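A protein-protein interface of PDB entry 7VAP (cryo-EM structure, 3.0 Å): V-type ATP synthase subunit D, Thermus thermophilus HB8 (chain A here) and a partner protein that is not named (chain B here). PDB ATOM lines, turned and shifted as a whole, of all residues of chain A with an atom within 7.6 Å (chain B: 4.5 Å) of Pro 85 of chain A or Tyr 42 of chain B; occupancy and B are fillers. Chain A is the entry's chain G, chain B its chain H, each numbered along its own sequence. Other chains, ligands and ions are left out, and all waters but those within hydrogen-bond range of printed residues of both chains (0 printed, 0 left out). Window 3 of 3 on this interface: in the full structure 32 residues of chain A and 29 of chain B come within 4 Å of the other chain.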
ATOM      1  N   ALA A  80     -16.226  16.608  -6.139  1.00  0.00           N
ATOM      2  CA  ALA A  80     -15.652  16.172  -7.409  1.00  0.00           C
ATOM      3  C   ALA A  80     -14.910  14.851  -7.254  1.00  0.00           C
ATOM      4  O   ALA A  80     -14.971  13.988  -8.139  1.00  0.00           O
ATOM      5  CB  ALA A  80     -14.720  17.250  -7.958  1.00  0.00           C
ATOM      6  N   LEU A  81     -14.196  14.678  -6.138  1.00  0.00           N
ATOM      7  CA  LEU A  81     -13.481  13.430  -5.896  1.00  0.00           C
ATOM      8  C   LEU A  81     -14.440  12.260  -5.740  1.00  0.00           C
ATOM      9  O   LEU A  81     -14.077  11.117  -6.040  1.00  0.00           O
ATOM     10  CB  LEU A  81     -12.597  13.562  -4.655  1.00  0.00           C
ATOM     11  CG  LEU A  81     -11.310  14.371  -4.829  1.00  0.00           C
ATOM     12  CD1 LEU A  81     -10.733  14.752  -3.476  1.00  0.00           C
ATOM     13  CD2 LEU A  81     -10.293  13.602  -5.658  1.00  0.00           C
ATOM     14  N   GLY A  82     -15.659  12.524  -5.269  1.00  0.00           N
ATOM     15  CA  GLY A  82     -16.649  11.462  -5.187  1.00  0.00           C
ATOM     16  C   GLY A  82     -16.956  10.849  -6.540  1.00  0.00           C
ATOM     17  O   GLY A  82     -17.132   9.633  -6.657  1.00  0.00           O
ATOM     18  N   VAL A  83     -17.022  11.674  -7.575  1.00  0.00           N
ATOM     19  CA  VAL A  83     -17.296  11.179  -8.925  1.00  0.00           C
ATOM     20  C   VAL A  83     -16.017  10.563  -9.491  1.00  0.00           C
ATOM     21  O   VAL A  83     -14.963  11.218  -9.468  1.00  0.00           O
ATOM     22  CB  VAL A  83     -17.805  12.306  -9.817  1.00  0.00           C
ATOM     23  CG1 VAL A  83     -17.999  11.805 -11.226  1.00  0.00           C
ATOM     24  CG2 VAL A  83     -19.107  12.869  -9.269  1.00  0.00           C
ATOM     25  N   PRO A  84     -16.062   9.332  -9.992  1.00  0.00           N
ATOM     26  CA  PRO A  84     -14.842   8.667 -10.448  1.00  0.00           C
ATOM     27  C   PRO A  84     -14.564   8.966 -11.910  1.00  0.00           C
ATOM     28  O   PRO A  84     -15.448   9.446 -12.635  1.00  0.00           O
ATOM     29  CB  PRO A  84     -15.167   7.184 -10.237  1.00  0.00           C
ATOM     30  CG  PRO A  84     -16.632   7.115 -10.527  1.00  0.00           C
ATOM     31  CD  PRO A  84     -17.229   8.436 -10.069  1.00  0.00           C
ATOM     32  N   PRO A  85     -13.340   8.702 -12.384  1.00  0.00           N
ATOM     33  CA  PRO A  85     -13.030   8.827 -13.826  1.00  0.00           C
ATOM     34  C   PRO A  85     -13.451   7.595 -14.625  1.00  0.00           C
ATOM     35  O   PRO A  85     -12.671   6.693 -14.933  1.00  0.00           O
ATOM     36  CB  PRO A  85     -11.513   9.023 -13.824  1.00  0.00           C
ATOM     37  CG  PRO A  85     -11.043   8.290 -12.615  1.00  0.00           C
ATOM     38  CD  PRO A  85     -12.146   8.367 -11.588  1.00  0.00           C
ATOM     39  N   LEU A  86     -14.733   7.554 -14.977  1.00  0.00           N
ATOM     40  CA  LEU A  86     -15.306   6.409 -15.665  1.00  0.00           C
ATOM     41  C   LEU A  86     -14.991   6.468 -17.159  1.00  0.00           C
ATOM     42  O   LEU A  86     -14.355   7.401 -17.656  1.00  0.00           O
ATOM     43  CB  LEU A  86     -16.813   6.355 -15.419  1.00  0.00           C
ATOM     44  CG  LEU A  86     -17.638   7.549 -15.913  1.00  0.00           C
ATOM     45  CD1 LEU A  86     -18.186   7.333 -17.322  1.00  0.00           C
ATOM     46  CD2 LEU A  86     -18.751   7.881 -14.940  1.00  0.00           C
ATOM     47  N   GLU A  87     -15.451   5.453 -17.886  1.00  0.00           N
ATOM     48  CA  GLU A  87     -15.352   5.413 -19.337  1.00  0.00           C
ATOM     49  C   GLU A  87     -16.751   5.326 -19.933  1.00  0.00           C
ATOM     50  O   GLU A  87     -17.651   4.711 -19.351  1.00  0.00           O
ATOM     51  CB  GLU A  87     -14.505   4.226 -19.820  1.00  0.00           C
ATOM     52  CG  GLU A  87     -15.189   2.870 -19.700  1.00  0.00           C
ATOM     53  CD  GLU A  87     -14.487   1.785 -20.492  1.00  0.00           C
ATOM     54  OE1 GLU A  87     -13.755   2.119 -21.449  1.00  0.00           O
ATOM     55  OE2 GLU A  87     -14.674   0.594 -20.165  1.00  0.00           O
ATOM     56  N   GLY A  88     -16.935   5.973 -21.079  1.00  0.00           N
ATOM     57  CA  GLY A  88     -18.180   5.871 -21.812  1.00  0.00           C
ATOM     58  C   GLY A  88     -17.957   5.863 -23.308  1.00  0.00           C
ATOM     59  O   GLY A  88     -18.913   5.820 -24.087  1.00  0.00           O
ATOM     60  N   VAL A  89     -16.693   5.895 -23.716  1.00  0.00           N
ATOM     61  CA  VAL A  89     -16.318   6.080 -25.113  1.00  0.00           C
ATOM     62  C   VAL A  89     -16.307   4.738 -25.829  1.00  0.00           C
ATOM     63  O   VAL A  89     -15.909   3.712 -25.264  1.00  0.00           O
ATOM     64  CB  VAL A  89     -14.950   6.781 -25.224  1.00  0.00           C
ATOM     65  CG1 VAL A  89     -15.062   8.237 -24.800  1.00  0.00           C
ATOM     66  CG2 VAL A  89     -13.906   6.057 -24.384  1.00  0.00           C
ATOM     67  N   LEU A 104     -15.377   8.517 -32.052  1.00  0.00           N
ATOM     68  CA  LEU A 104     -15.621   8.405 -30.615  1.00  0.00           C
ATOM     69  C   LEU A 104     -17.126   8.457 -30.350  1.00  0.00           C
ATOM     70  O   LEU A 104     -17.669   9.403 -29.778  1.00  0.00           O
ATOM     71  CB  LEU A 104     -14.867   9.494 -29.863  1.00  0.00           C
ATOM     72  CG  LEU A 104     -13.344   9.369 -29.955  1.00  0.00           C
ATOM     73  CD1 LEU A 104     -12.653  10.557 -29.314  1.00  0.00           C
ATOM     74  CD2 LEU A 104     -12.876   8.075 -29.313  1.00  0.00           C
ATOM     75  N   ALA A 112     -23.347   6.056 -14.619  1.00  0.00           N
ATOM     76  CA  ALA A 112     -22.067   5.461 -14.263  1.00  0.00           C
ATOM     77  C   ALA A 112     -21.274   6.307 -13.278  1.00  0.00           C
ATOM     78  O   ALA A 112     -20.256   5.835 -12.759  1.00  0.00           O
ATOM     79  CB  ALA A 112     -21.230   5.219 -15.525  1.00  0.00           C
ATOM     80  N   LEU A 114     -20.319   7.325 -10.055  1.00  0.00           N
ATOM     81  CA  LEU A 114     -20.457   6.945  -8.656  1.00  0.00           C
ATOM     82  C   LEU A 114     -20.392   8.182  -7.768  1.00  0.00           C
ATOM     83  O   LEU A 114     -19.640   9.121  -8.041  1.00  0.00           O
ATOM     84  CB  LEU A 114     -19.365   5.952  -8.255  1.00  0.00           C
ATOM     85  CG  LEU A 114     -19.627   4.462  -8.504  1.00  0.00           C
ATOM     86  CD1 LEU A 114     -20.850   3.997  -7.722  1.00  0.00           C
ATOM     87  CD2 LEU A 114     -19.768   4.140  -9.987  1.00  0.00           C
ATOM     88  N   MET B   1     -11.408   8.579 -21.874  1.00  0.00           N
ATOM     89  CA  MET B   1     -10.968   9.939 -22.157  1.00  0.00           C
ATOM     90  C   MET B   1     -10.153  10.499 -20.995  1.00  0.00           C
ATOM     91  O   MET B   1     -10.256  10.017 -19.867  1.00  0.00           O
ATOM     92  CB  MET B   1     -12.169  10.839 -22.440  1.00  0.00           C
ATOM     93  CG  MET B   1     -12.942  11.227 -21.196  1.00  0.00           C
ATOM     94  SD  MET B   1     -13.428   9.812 -20.184  1.00  0.00           S
ATOM     95  CE  MET B   1     -14.576   8.980 -21.276  1.00  0.00           C
ATOM     96  N   ALA B   2      -9.343  11.518 -21.273  1.00  0.00           N
ATOM     97  CA  ALA B   2      -8.537  12.152 -20.241  1.00  0.00           C
ATOM     98  C   ALA B   2      -8.198  13.571 -20.671  1.00  0.00           C
ATOM     99  O   ALA B   2      -8.203  13.893 -21.862  1.00  0.00           O
ATOM    100  CB  ALA B   2      -7.256  11.359 -19.957  1.00  0.00           C
ATOM    101  N   ARG B  14     -13.001  15.680 -13.344  1.00  0.00           N
ATOM    102  CA  ARG B  14     -13.242  14.540 -12.464  1.00  0.00           C
ATOM    103  C   ARG B  14     -14.679  14.537 -11.954  1.00  0.00           C
ATOM    104  O   ARG B  14     -15.303  13.477 -11.835  1.00  0.00           O
ATOM    105  CB  ARG B  14     -12.253  14.550 -11.298  1.00  0.00           C
ATOM    106  CG  ARG B  14     -12.452  13.404 -10.319  1.00  0.00           C
ATOM    107  CD  ARG B  14     -12.324  12.053 -11.010  1.00  0.00           C
ATOM    108  NE  ARG B  14     -10.954  11.749 -11.409  1.00  0.00           N
ATOM    109  CZ  ARG B  14     -10.000  11.358 -10.574  1.00  0.00           C
ATOM    110  NH1 ARG B  14     -10.231  11.210  -9.281  1.00  0.00           N
ATOM    111  NH2 ARG B  14      -8.785  11.105 -11.053  1.00  0.00           N
ATOM    112  N   GLY B  17     -17.219  13.054 -14.277  1.00  0.00           N
ATOM    113  CA  GLY B  17     -17.064  11.643 -14.541  1.00  0.00           C
ATOM    114  C   GLY B  17     -15.892  11.299 -15.424  1.00  0.00           C
ATOM    115  O   GLY B  17     -15.761  10.139 -15.827  1.00  0.00           O
ATOM    116  N   LEU B  18     -15.037  12.265 -15.731  1.00  0.00           N
ATOM    117  CA  LEU B  18     -13.937  12.096 -16.661  1.00  0.00           C
ATOM    118  C   LEU B  18     -12.641  11.917 -15.877  1.00  0.00           C
ATOM    119  O   LEU B  18     -12.622  11.930 -14.644  1.00  0.00           O
ATOM    120  CB  LEU B  18     -13.850  13.302 -17.598  1.00  0.00           C
ATOM    121  CG  LEU B  18     -15.104  13.648 -18.410  1.00  0.00           C
ATOM    122  CD1 LEU B  18     -14.859  14.893 -19.252  1.00  0.00           C
ATOM    123  CD2 LEU B  18     -15.602  12.489 -19.264  1.00  0.00           C
ATOM    124  N   GLU B  19     -11.544  11.757 -16.608  1.00  0.00           N
ATOM    125  CA  GLU B  19     -10.219  11.694 -16.011  1.00  0.00           C
ATOM    126  C   GLU B  19      -9.478  12.997 -16.273  1.00  0.00           C
ATOM    127  O   GLU B  19      -9.481  13.513 -17.396  1.00  0.00           O
ATOM    128  CB  GLU B  19      -9.418  10.512 -16.563  1.00  0.00           C
ATOM    129  CG  GLU B  19      -8.058  10.300 -15.900  1.00  0.00           C
ATOM    130  CD  GLU B  19      -8.163   9.883 -14.445  1.00  0.00           C
ATOM    131  OE1 GLU B  19      -8.412  10.752 -13.582  1.00  0.00           O
ATOM    132  OE2 GLU B  19      -7.994   8.678 -14.159  1.00  0.00           O
ATOM    133  N   ARG B  39       0.628   4.739 -20.896  1.00  0.00           N
ATOM    134  CA  ARG B  39      -0.405   4.013 -20.171  1.00  0.00           C
ATOM    135  C   ARG B  39      -1.476   3.506 -21.132  1.00  0.00           C
ATOM    136  O   ARG B  39      -2.080   4.288 -21.873  1.00  0.00           O
ATOM    137  CB  ARG B  39      -1.029   4.918 -19.108  1.00  0.00           C
ATOM    138  CG  ARG B  39      -2.139   4.272 -18.291  1.00  0.00           C
ATOM    139  CD  ARG B  39      -3.513   4.662 -18.818  1.00  0.00           C
ATOM    140  NE  ARG B  39      -3.678   6.109 -18.912  1.00  0.00           N
ATOM    141  CZ  ARG B  39      -4.631   6.707 -19.612  1.00  0.00           C
ATOM    142  NH1 ARG B  39      -5.507   6.011 -20.317  1.00  0.00           N
ATOM    143  NH2 ARG B  39      -4.703   8.034 -19.610  1.00  0.00           N
ATOM    144  N   GLY B  41      -5.045   2.450 -22.129  1.00  0.00           N
ATOM    145  CA  GLY B  41      -6.315   2.915 -21.609  1.00  0.00           C
ATOM    146  C   GLY B  41      -7.135   3.751 -22.569  1.00  0.00           C
ATOM    147  O   GLY B  41      -7.433   3.321 -23.688  1.00  0.00           O
ATOM    148  N   TYR B  42      -7.518   4.945 -22.118  1.00  0.00           N
ATOM    149  CA  TYR B  42      -8.426   5.824 -22.841  1.00  0.00           C
ATOM    150  C   TYR B  42      -7.931   6.114 -24.256  1.00  0.00           C
ATOM    151  O   TYR B  42      -6.758   5.929 -24.591  1.00  0.00           O
ATOM    152  CB  TYR B  42      -8.593   7.146 -22.095  1.00  0.00           C
ATOM    153  CG  TYR B  42      -8.761   7.011 -20.598  1.00  0.00           C
ATOM    154  CD1 TYR B  42      -9.624   6.069 -20.053  1.00  0.00           C
ATOM    155  CD2 TYR B  42      -8.048   7.827 -19.728  1.00  0.00           C
ATOM    156  CE1 TYR B  42      -9.774   5.946 -18.686  1.00  0.00           C
ATOM    157  CE2 TYR B  42      -8.191   7.711 -18.363  1.00  0.00           C
ATOM    158  CZ  TYR B  42      -9.055   6.771 -17.846  1.00  0.00           C
ATOM    159  OH  TYR B  42      -9.196   6.656 -16.482  1.00  0.00           O
ATOM    160  N   ALA B  43      -8.855   6.591 -25.088  1.00  0.00           N
ATOM    161  CA  ALA B  43      -8.564   6.949 -26.467  1.00  0.00           C
ATOM    162  C   ALA B  43      -8.699   8.441 -26.742  1.00  0.00           C
ATOM    163  O   ALA B  43      -8.539   8.858 -27.892  1.00  0.00           O
ATOM    164  CB  ALA B  43      -9.476   6.167 -27.419  1.00  0.00           C
ATOM    165  N   LEU B  44      -8.994   9.252 -25.729  1.00  0.00           N
ATOM    166  CA  LEU B  44      -9.127  10.695 -25.895  1.00  0.00           C
ATOM    167  C   LEU B  44      -8.215  11.397 -24.903  1.00  0.00           C
ATOM    168  O   LEU B  44      -8.206  11.059 -23.716  1.00  0.00           O
ATOM    169  CB  LEU B  44     -10.577  11.159 -25.695  1.00  0.00           C
ATOM    170  CG  LEU B  44     -10.885  12.640 -25.952  1.00  0.00           C
ATOM    171  CD1 LEU B  44     -12.273  12.803 -26.541  1.00  0.00           C
ATOM    172  CD2 LEU B  44     -10.765  13.474 -24.681  1.00  0.00           C
ATOM    173  N   PRO B  69      -5.063   6.949 -28.780  1.00  0.00           N
ATOM    174  CA  PRO B  69      -5.377   8.169 -28.016  1.00  0.00           C
ATOM    175  C   PRO B  69      -5.548   9.363 -28.944  1.00  0.00           C
ATOM    176  O   PRO B  69      -4.637   9.716 -29.695  1.00  0.00           O
ATOM    177  CB  PRO B  69      -4.163   8.339 -27.094  1.00  0.00           C
ATOM    178  CG  PRO B  69      -3.504   7.008 -27.066  1.00  0.00           C
ATOM    179  CD  PRO B  69      -3.733   6.427 -28.420  1.00  0.00           C
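The backbone carbonyl oxygen of Leu 86 of chain A sits close to the side-chain sulfur of Met 1 of chain B (3.6 Å).
The backbone carbonyl oxygen (O) of Gly 17 of chain B sits at hydrogen-bond distance from the backbone NH (N) of Leu 86 of chain A.
O of Arg 14 of chain B sits close to O of Val 83 of chain A (3.3 Å).
O of Gly 17 of chain B sits close to O of Pro 84 of chain A, at 3.3 Å.
Of the printed residues of chain B, Ala 80 of chain A touches Arg 14 (3.4 Å).
Leu 81 of chain A touches none of the printed residues of chain B.
Of the printed residues of chain B, Pro 84 of chain A touches Arg 14 (3.9 Å) and Gly 17 (3.3 Å).
Pro 85 of chain A touches five residues of chain B.
Leu 114 of chain A touches none of the printed residues of chain B.
Of the printed residues of chain A, Leu 18 of chain B touches Pro 85.
Of chain A, only Pro 85 (3.8 Å) comes within 4 Å of Tyr 42 of chain B.
The nearest printed residue of chain B that does not touch Pro 85 of chain A is Met 1 of chain B (6.0 Å).
The nearest residue of chain A that does not touch Tyr 42 of chain B is Leu 86 of chain A (4.9 Å).
The nearest printed residue of chain A that does not touch Arg 14 of chain B is Leu 81 of chain A (4.3 Å).
OE1 of Glu 19 of chain B lies within salt-bridge range of NH2 of Arg 14 of chain B (2.6 Å).
The side-chain carboxylate (OE2) of Glu 19 of chain B sits at hydrogen-bond distance from the side-chain hydroxyl (OH) of Tyr 42 of chain B (3.3 Å).
N of Ala 2 of chain B lies within hydrogen-bond range of O of Leu 44 of chain B (2.7 Å).
Hydrophobic or aromatic side chains of chain A that line the printed part of chain B: Val 83, Pro 85, Leu 86, Val 89 and Leu 104.
Of the 12 printed residues of chain B, 7 touch a printed residue of chain A.
Hydrophobic or aromatic side chains of chain B within 4 Å of the printed part of chain A: Met 1, Tyr 42 and Leu 44.
Along chain B the printed residues that touch a printed residue of chain A span positions 1 to 44.
Among the printed residues, 15 pairs touch across the chains.
Among the printed residues, no Asp or Glu carboxylate lies within 4 Å of a Lys or Arg side-chain nitrogen of the other chain.
O of Ala 80 of chain A touches CG of Arg 14 of chain B, 3.4 Å away.
Val 83 of chain A touches Gly 17 of chain B (CG1 to N, 3.4 Å).
Pro 84 of chain A touches Arg 14 of chain B.
Arg 14 of chain B touches Pro 85 of chain A (NE to CD, 3.6 Å).
Leu 18 of chain B touches Pro 85 of chain A.
Glu 19 of chain B touches Pro 85 of chain A (OE2 to CG, 3.4 Å).
Tyr 42 of chain B touches Pro 85 of chain A.
Met 1 of chain B touches Gly 88 of chain A.
CG1 of Val 89 of chain A touches CE of Met 1 of chain B (3.6 Å).
Leu 44 of chain B touches Leu 104 of chain A.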
